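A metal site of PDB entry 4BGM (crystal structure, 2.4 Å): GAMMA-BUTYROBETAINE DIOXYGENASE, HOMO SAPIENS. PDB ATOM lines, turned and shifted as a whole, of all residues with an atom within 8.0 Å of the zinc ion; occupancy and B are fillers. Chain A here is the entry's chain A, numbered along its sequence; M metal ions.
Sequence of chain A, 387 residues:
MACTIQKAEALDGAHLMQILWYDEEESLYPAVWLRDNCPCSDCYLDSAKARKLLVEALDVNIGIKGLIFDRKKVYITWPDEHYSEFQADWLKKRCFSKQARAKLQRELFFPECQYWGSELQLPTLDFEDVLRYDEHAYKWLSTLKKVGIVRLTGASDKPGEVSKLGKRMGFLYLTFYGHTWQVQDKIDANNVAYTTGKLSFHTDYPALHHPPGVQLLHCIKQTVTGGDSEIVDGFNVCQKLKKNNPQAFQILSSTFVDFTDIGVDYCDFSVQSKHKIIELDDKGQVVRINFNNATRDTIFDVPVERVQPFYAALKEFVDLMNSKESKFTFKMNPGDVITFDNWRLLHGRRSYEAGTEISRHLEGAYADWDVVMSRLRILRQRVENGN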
ATOM      1  N   LEU A  34     -18.947 -14.935  -6.345  1.00  0.00           N
ATOM      2  CA  LEU A  34     -19.705 -14.014  -5.495  1.00  0.00           C
ATOM      3  C   LEU A  34     -19.755 -14.582  -4.082  1.00  0.00           C
ATOM      4  O   LEU A  34     -19.449 -13.893  -3.115  1.00  0.00           O
ATOM      5  CB  LEU A  34     -21.136 -13.827  -6.022  1.00  0.00           C
ATOM      6  CG  LEU A  34     -21.285 -13.120  -7.373  1.00  0.00           C
ATOM      7  CD1 LEU A  34     -22.696 -13.333  -7.933  1.00  0.00           C
ATOM      8  CD2 LEU A  34     -20.962 -11.637  -7.235  1.00  0.00           C
ATOM      9  N   ARG A  35     -20.095 -15.847  -3.961  1.00  0.00           N
ATOM     10  CA  ARG A  35     -20.134 -16.461  -2.671  1.00  0.00           C
ATOM     11  C   ARG A  35     -18.775 -16.448  -1.982  1.00  0.00           C
ATOM     12  O   ARG A  35     -18.686 -16.258  -0.769  1.00  0.00           O
ATOM     13  CB  ARG A  35     -20.631 -17.897  -2.771  1.00  0.00           C
ATOM     14  CG  ARG A  35     -20.731 -18.611  -1.419  1.00  0.00           C
ATOM     15  CD  ARG A  35     -21.686 -17.853  -0.486  1.00  0.00           C
ATOM     16  NE  ARG A  35     -21.794 -18.416   0.863  1.00  0.00           N
ATOM     17  CZ  ARG A  35     -21.064 -18.026   1.872  1.00  0.00           C
ATOM     18  NH1 ARG A  35     -20.167 -17.068   1.682  1.00  0.00           N
ATOM     19  NH2 ARG A  35     -21.222 -18.574   3.061  1.00  0.00           N
ATOM     20  N   ASP A  36     -17.724 -16.686  -2.765  1.00  0.00           N
ATOM     21  CA  ASP A  36     -16.360 -16.788  -2.206  1.00  0.00           C
ATOM     22  C   ASP A  36     -15.963 -15.431  -1.607  1.00  0.00           C
ATOM     23  O   ASP A  36     -15.267 -15.373  -0.575  1.00  0.00           O
ATOM     24  CB  ASP A  36     -15.399 -17.202  -3.315  1.00  0.00           C
ATOM     25  CG  ASP A  36     -13.961 -17.206  -2.880  1.00  0.00           C
ATOM     26  OD1 ASP A  36     -13.618 -17.831  -1.806  1.00  0.00           O
ATOM     27  OD2 ASP A  36     -13.175 -16.573  -3.635  1.00  0.00           O
ATOM     28  N   ASN A  37     -16.464 -14.354  -2.231  1.00  0.00           N
ATOM     29  CA  ASN A  37     -16.111 -12.988  -1.850  1.00  0.00           C
ATOM     30  C   ASN A  37     -17.215 -12.192  -1.166  1.00  0.00           C
ATOM     31  O   ASN A  37     -17.246 -10.965  -1.258  1.00  0.00           O
ATOM     32  CB  ASN A  37     -15.591 -12.269  -3.065  1.00  0.00           C
ATOM     33  CG  ASN A  37     -14.275 -12.819  -3.520  1.00  0.00           C
ATOM     34  OD1 ASN A  37     -13.284 -12.766  -2.770  1.00  0.00           O
ATOM     35  ND2 ASN A  37     -14.248 -13.408  -4.723  1.00  0.00           N
ATOM     36  N   CYS A  38     -18.077 -12.895  -0.427  1.00  0.00           N
ATOM     37  CA  CYS A  38     -19.084 -12.220   0.378  1.00  0.00           C
ATOM     38  C   CYS A  38     -18.401 -11.300   1.391  1.00  0.00           C
ATOM     39  O   CYS A  38     -17.586 -11.744   2.170  1.00  0.00           O
ATOM     40  CB  CYS A  38     -19.979 -13.237   1.118  1.00  0.00           C
ATOM     41  SG  CYS A  38     -21.179 -12.454   2.244  1.00  0.00           S
ATOM     42  N   PRO A  39     -18.738 -10.013   1.390  1.00  0.00           N
ATOM     43  CA  PRO A  39     -18.107  -9.108   2.352  1.00  0.00           C
ATOM     44  C   PRO A  39     -18.708  -9.114   3.759  1.00  0.00           C
ATOM     45  O   PRO A  39     -18.373  -8.241   4.549  1.00  0.00           O
ATOM     46  CB  PRO A  39     -18.296  -7.733   1.711  1.00  0.00           C
ATOM     47  CG  PRO A  39     -19.561  -7.866   0.940  1.00  0.00           C
ATOM     48  CD  PRO A  39     -19.581  -9.278   0.419  1.00  0.00           C
ATOM     49  N   CYS A  40     -19.601 -10.043   4.078  1.00  0.00           N
ATOM     50  CA  CYS A  40     -20.250 -10.039   5.384  1.00  0.00           C
ATOM     51  C   CYS A  40     -19.202 -10.355   6.483  1.00  0.00           C
ATOM     52  O   CYS A  40     -18.121 -10.899   6.198  1.00  0.00           O
ATOM     53  CB  CYS A  40     -21.464 -11.016   5.401  1.00  0.00           C
ATOM     54  SG  CYS A  40     -21.142 -12.707   6.010  1.00  0.00           S
ATOM     55  N   SER A  41     -19.500 -10.031   7.729  1.00  0.00           N
ATOM     56  CA  SER A  41     -18.552 -10.217   8.828  1.00  0.00           C
ATOM     57  C   SER A  41     -18.249 -11.696   9.152  1.00  0.00           C
ATOM     58  O   SER A  41     -17.249 -11.985   9.824  1.00  0.00           O
ATOM     59  CB  SER A  41     -19.012  -9.463  10.101  1.00  0.00           C
ATOM     60  OG  SER A  41     -20.100 -10.103  10.735  1.00  0.00           O
ATOM     61  N   ASP A  42     -19.081 -12.633   8.699  1.00  0.00           N
ATOM     62  CA  ASP A  42     -18.734 -14.074   8.842  1.00  0.00           C
ATOM     63  C   ASP A  42     -17.663 -14.519   7.852  1.00  0.00           C
ATOM     64  O   ASP A  42     -16.772 -15.315   8.205  1.00  0.00           O
ATOM     65  CB  ASP A  42     -19.951 -14.977   8.640  1.00  0.00           C
ATOM     66  CG  ASP A  42     -20.979 -14.832   9.735  1.00  0.00           C
ATOM     67  OD1 ASP A  42     -20.720 -14.112  10.740  1.00  0.00           O
ATOM     68  OD2 ASP A  42     -22.034 -15.449   9.602  1.00  0.00           O
ATOM     69  N   CYS A  43     -17.743 -13.998   6.624  1.00  0.00           N
ATOM     70  CA  CYS A  43     -16.895 -14.422   5.516  1.00  0.00           C
ATOM     71  C   CYS A  43     -15.633 -13.585   5.291  1.00  0.00           C
ATOM     72  O   CYS A  43     -14.754 -14.006   4.552  1.00  0.00           O
ATOM     73  CB  CYS A  43     -17.710 -14.376   4.216  1.00  0.00           C
ATOM     74  SG  CYS A  43     -19.174 -15.409   4.250  1.00  0.00           S
ATOM     75  N   TYR A  44     -15.578 -12.413   5.919  1.00  0.00           N
ATOM     76  CA  TYR A  44     -14.580 -11.406   5.623  1.00  0.00           C
ATOM     77  C   TYR A  44     -14.201 -10.552   6.862  1.00  0.00           C
ATOM     78  O   TYR A  44     -15.065  -9.937   7.510  1.00  0.00           O
ATOM     79  CB  TYR A  44     -15.069 -10.507   4.485  1.00  0.00           C
ATOM     80  CG  TYR A  44     -14.013  -9.614   3.860  1.00  0.00           C
ATOM     81  CD1 TYR A  44     -13.195 -10.085   2.847  1.00  0.00           C
ATOM     82  CD2 TYR A  44     -13.834  -8.292   4.283  1.00  0.00           C
ATOM     83  CE1 TYR A  44     -12.233  -9.288   2.258  1.00  0.00           C
ATOM     84  CE2 TYR A  44     -12.867  -7.474   3.701  1.00  0.00           C
ATOM     85  CZ  TYR A  44     -12.069  -7.982   2.685  1.00  0.00           C
ATOM     86  OH  TYR A  44     -11.100  -7.205   2.090  1.00  0.00           O
ATOM     87  N   LEU A  53     -13.727 -16.794   5.078  1.00  0.00           N
ATOM     88  CA  LEU A  53     -14.326 -17.959   4.419  1.00  0.00           C
ATOM     89  C   LEU A  53     -13.281 -19.020   4.019  1.00  0.00           C
ATOM     90  O   LEU A  53     -12.328 -18.714   3.335  1.00  0.00           O
ATOM     91  CB  LEU A  53     -15.101 -17.511   3.185  1.00  0.00           C
ATOM     92  CG  LEU A  53     -16.032 -18.542   2.582  1.00  0.00           C
ATOM     93  CD1 LEU A  53     -17.130 -18.967   3.546  1.00  0.00           C
ATOM     94  CD2 LEU A  53     -16.615 -17.940   1.329  1.00  0.00           C
ATOM     95  N   TRP A  78     -28.518 -17.278  -0.751  1.00  0.00           N
ATOM     96  CA  TRP A  78     -27.885 -18.501  -1.209  1.00  0.00           C
ATOM     97  C   TRP A  78     -28.689 -19.734  -0.757  1.00  0.00           C
ATOM     98  O   TRP A  78     -29.395 -19.674   0.232  1.00  0.00           O
ATOM     99  CB  TRP A  78     -26.437 -18.561  -0.648  1.00  0.00           C
ATOM    100  CG  TRP A  78     -25.550 -17.436  -1.147  1.00  0.00           C
ATOM    101  CD1 TRP A  78     -25.132 -16.360  -0.438  1.00  0.00           C
ATOM    102  CD2 TRP A  78     -25.022 -17.274  -2.470  1.00  0.00           C
ATOM    103  NE1 TRP A  78     -24.365 -15.534  -1.235  1.00  0.00           N
ATOM    104  CE2 TRP A  78     -24.278 -16.073  -2.482  1.00  0.00           C
ATOM    105  CE3 TRP A  78     -25.110 -18.012  -3.652  1.00  0.00           C
ATOM    106  CZ2 TRP A  78     -23.634 -15.607  -3.630  1.00  0.00           C
ATOM    107  CZ3 TRP A  78     -24.438 -17.554  -4.786  1.00  0.00           C
ATOM    108  CH2 TRP A  78     -23.712 -16.371  -4.759  1.00  0.00           C
ATOM    109  N   HIS A  82     -27.440 -18.405   3.605  1.00  0.00           N
ATOM    110  CA  HIS A  82     -26.484 -17.329   3.765  1.00  0.00           C
ATOM    111  C   HIS A  82     -26.943 -16.135   2.904  1.00  0.00           C
ATOM    112  O   HIS A  82     -27.656 -16.325   1.914  1.00  0.00           O
ATOM    113  CB  HIS A  82     -25.083 -17.802   3.383  1.00  0.00           C
ATOM    114  CG  HIS A  82     -24.008 -16.871   3.817  1.00  0.00           C
ATOM    115  ND1 HIS A  82     -23.496 -16.882   5.091  1.00  0.00           N
ATOM    116  CD2 HIS A  82     -23.399 -15.839   3.180  1.00  0.00           C
ATOM    117  CE1 HIS A  82     -22.606 -15.920   5.213  1.00  0.00           C
ATOM    118  NE2 HIS A  82     -22.531 -15.273   4.066  1.00  0.00           N
ATOM    119  N   TYR A  83     -26.556 -14.921   3.308  1.00  0.00           N
ATOM    120  CA  TYR A  83     -27.048 -13.700   2.659  1.00  0.00           C
ATOM    121  C   TYR A  83     -25.892 -12.757   2.346  1.00  0.00           C
ATOM    122  O   TYR A  83     -25.025 -12.545   3.188  1.00  0.00           O
ATOM    123  CB  TYR A  83     -28.068 -13.004   3.602  1.00  0.00           C
ATOM    124  CG  TYR A  83     -28.458 -11.612   3.153  1.00  0.00           C
ATOM    125  CD1 TYR A  83     -29.239 -11.436   2.016  1.00  0.00           C
ATOM    126  CD2 TYR A  83     -28.017 -10.474   3.832  1.00  0.00           C
ATOM    127  CE1 TYR A  83     -29.594 -10.162   1.578  1.00  0.00           C
ATOM    128  CE2 TYR A  83     -28.343  -9.183   3.391  1.00  0.00           C
ATOM    129  CZ  TYR A  83     -29.147  -9.036   2.274  1.00  0.00           C
ATOM    130  OH  TYR A  83     -29.508  -7.766   1.824  1.00  0.00           O
ATOM    131  N   SER A  84     -25.876 -12.186   1.146  1.00  0.00           N
ATOM    132  CA  SER A  84     -24.734 -11.386   0.688  1.00  0.00           C
ATOM    133  C   SER A  84     -25.167 -10.082   0.001  1.00  0.00           C
ATOM    134  O   SER A  84     -26.102 -10.079  -0.818  1.00  0.00           O
ATOM    135  CB  SER A  84     -23.846 -12.209  -0.281  1.00  0.00           C
ATOM    136  OG  SER A  84     -23.351 -13.412   0.327  1.00  0.00           O
ATOM    137  N   GLU A  85     -24.495  -8.989   0.328  1.00  0.00           N
ATOM    138  CA  GLU A  85     -24.732  -7.700  -0.319  1.00  0.00           C
ATOM    139  C   GLU A  85     -23.463  -7.224  -0.983  1.00  0.00           C
ATOM    140  O   GLU A  85     -22.397  -7.270  -0.362  1.00  0.00           O
ATOM    141  CB  GLU A  85     -25.110  -6.641   0.719  1.00  0.00           C
ATOM    142  CG  GLU A  85     -26.227  -7.037   1.659  1.00  0.00           C
ATOM    143  CD  GLU A  85     -26.803  -5.816   2.360  1.00  0.00           C
ATOM    144  OE1 GLU A  85     -26.108  -4.783   2.351  1.00  0.00           O
ATOM    145  OE2 GLU A  85     -27.949  -5.894   2.871  1.00  0.00           O
ATOM    146  N   PHE A  86     -23.579  -6.757  -2.209  1.00  0.00           N
ATOM    147  CA  PHE A  86     -22.416  -6.239  -2.956  1.00  0.00           C
ATOM    148  C   PHE A  86     -22.670  -4.851  -3.504  1.00  0.00           C
ATOM    149  O   PHE A  86     -23.769  -4.549  -3.953  1.00  0.00           O
ATOM    150  CB  PHE A  86     -22.077  -7.152  -4.128  1.00  0.00           C
ATOM    151  CG  PHE A  86     -21.843  -8.589  -3.752  1.00  0.00           C
ATOM    152  CD1 PHE A  86     -20.569  -9.037  -3.425  1.00  0.00           C
ATOM    153  CD2 PHE A  86     -22.888  -9.509  -3.811  1.00  0.00           C
ATOM    154  CE1 PHE A  86     -20.359 -10.358  -3.106  1.00  0.00           C
ATOM    155  CE2 PHE A  86     -22.669 -10.842  -3.509  1.00  0.00           C
ATOM    156  CZ  PHE A  86     -21.413 -11.259  -3.142  1.00  0.00           C
HETATM  157 ZN    ZN M   1     -20.981 -13.819   4.063  1.00  0.00          ZN
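A ring nitrogen (ND1) of His 82 sits close to the guanidinium group (NH2) of Arg 35 (3.5 Å). The backbone NH (N) of Asp 42 lies close to the side-chain sulfur (SG) of Cys 40 (3.4 Å). The side-chain sulfur (SG) of Cys 38 sits close to the side-chain hydroxyl (OG) of Ser 84. The side-chain sulfur (SG) of Cys 43 sits close to the guanidinium group (NH1) of Arg 35 (3.2 Å). The backbone carbonyl oxygen (O) of Cys 43 is in hydrogen-bond range of the backbone NH (N) of Leu 53, at 3.0 Å.
The zinc ion is bound by NE2 of His 82 (2.1 Å), SG of Cys 40 (2.2 Å), SG of Cys 38 (2.3 Å) and SG of Cys 43 (2.4 Å). The zinc ion has four donor atoms within binding distance.
Four residues have an atom within 4 Å of the zinc ion: Cys 38, Cys 40, Cys 43 and His 82. The nearest printed residue that does not touch the zinc ion is Arg 35 (4.1 Å).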
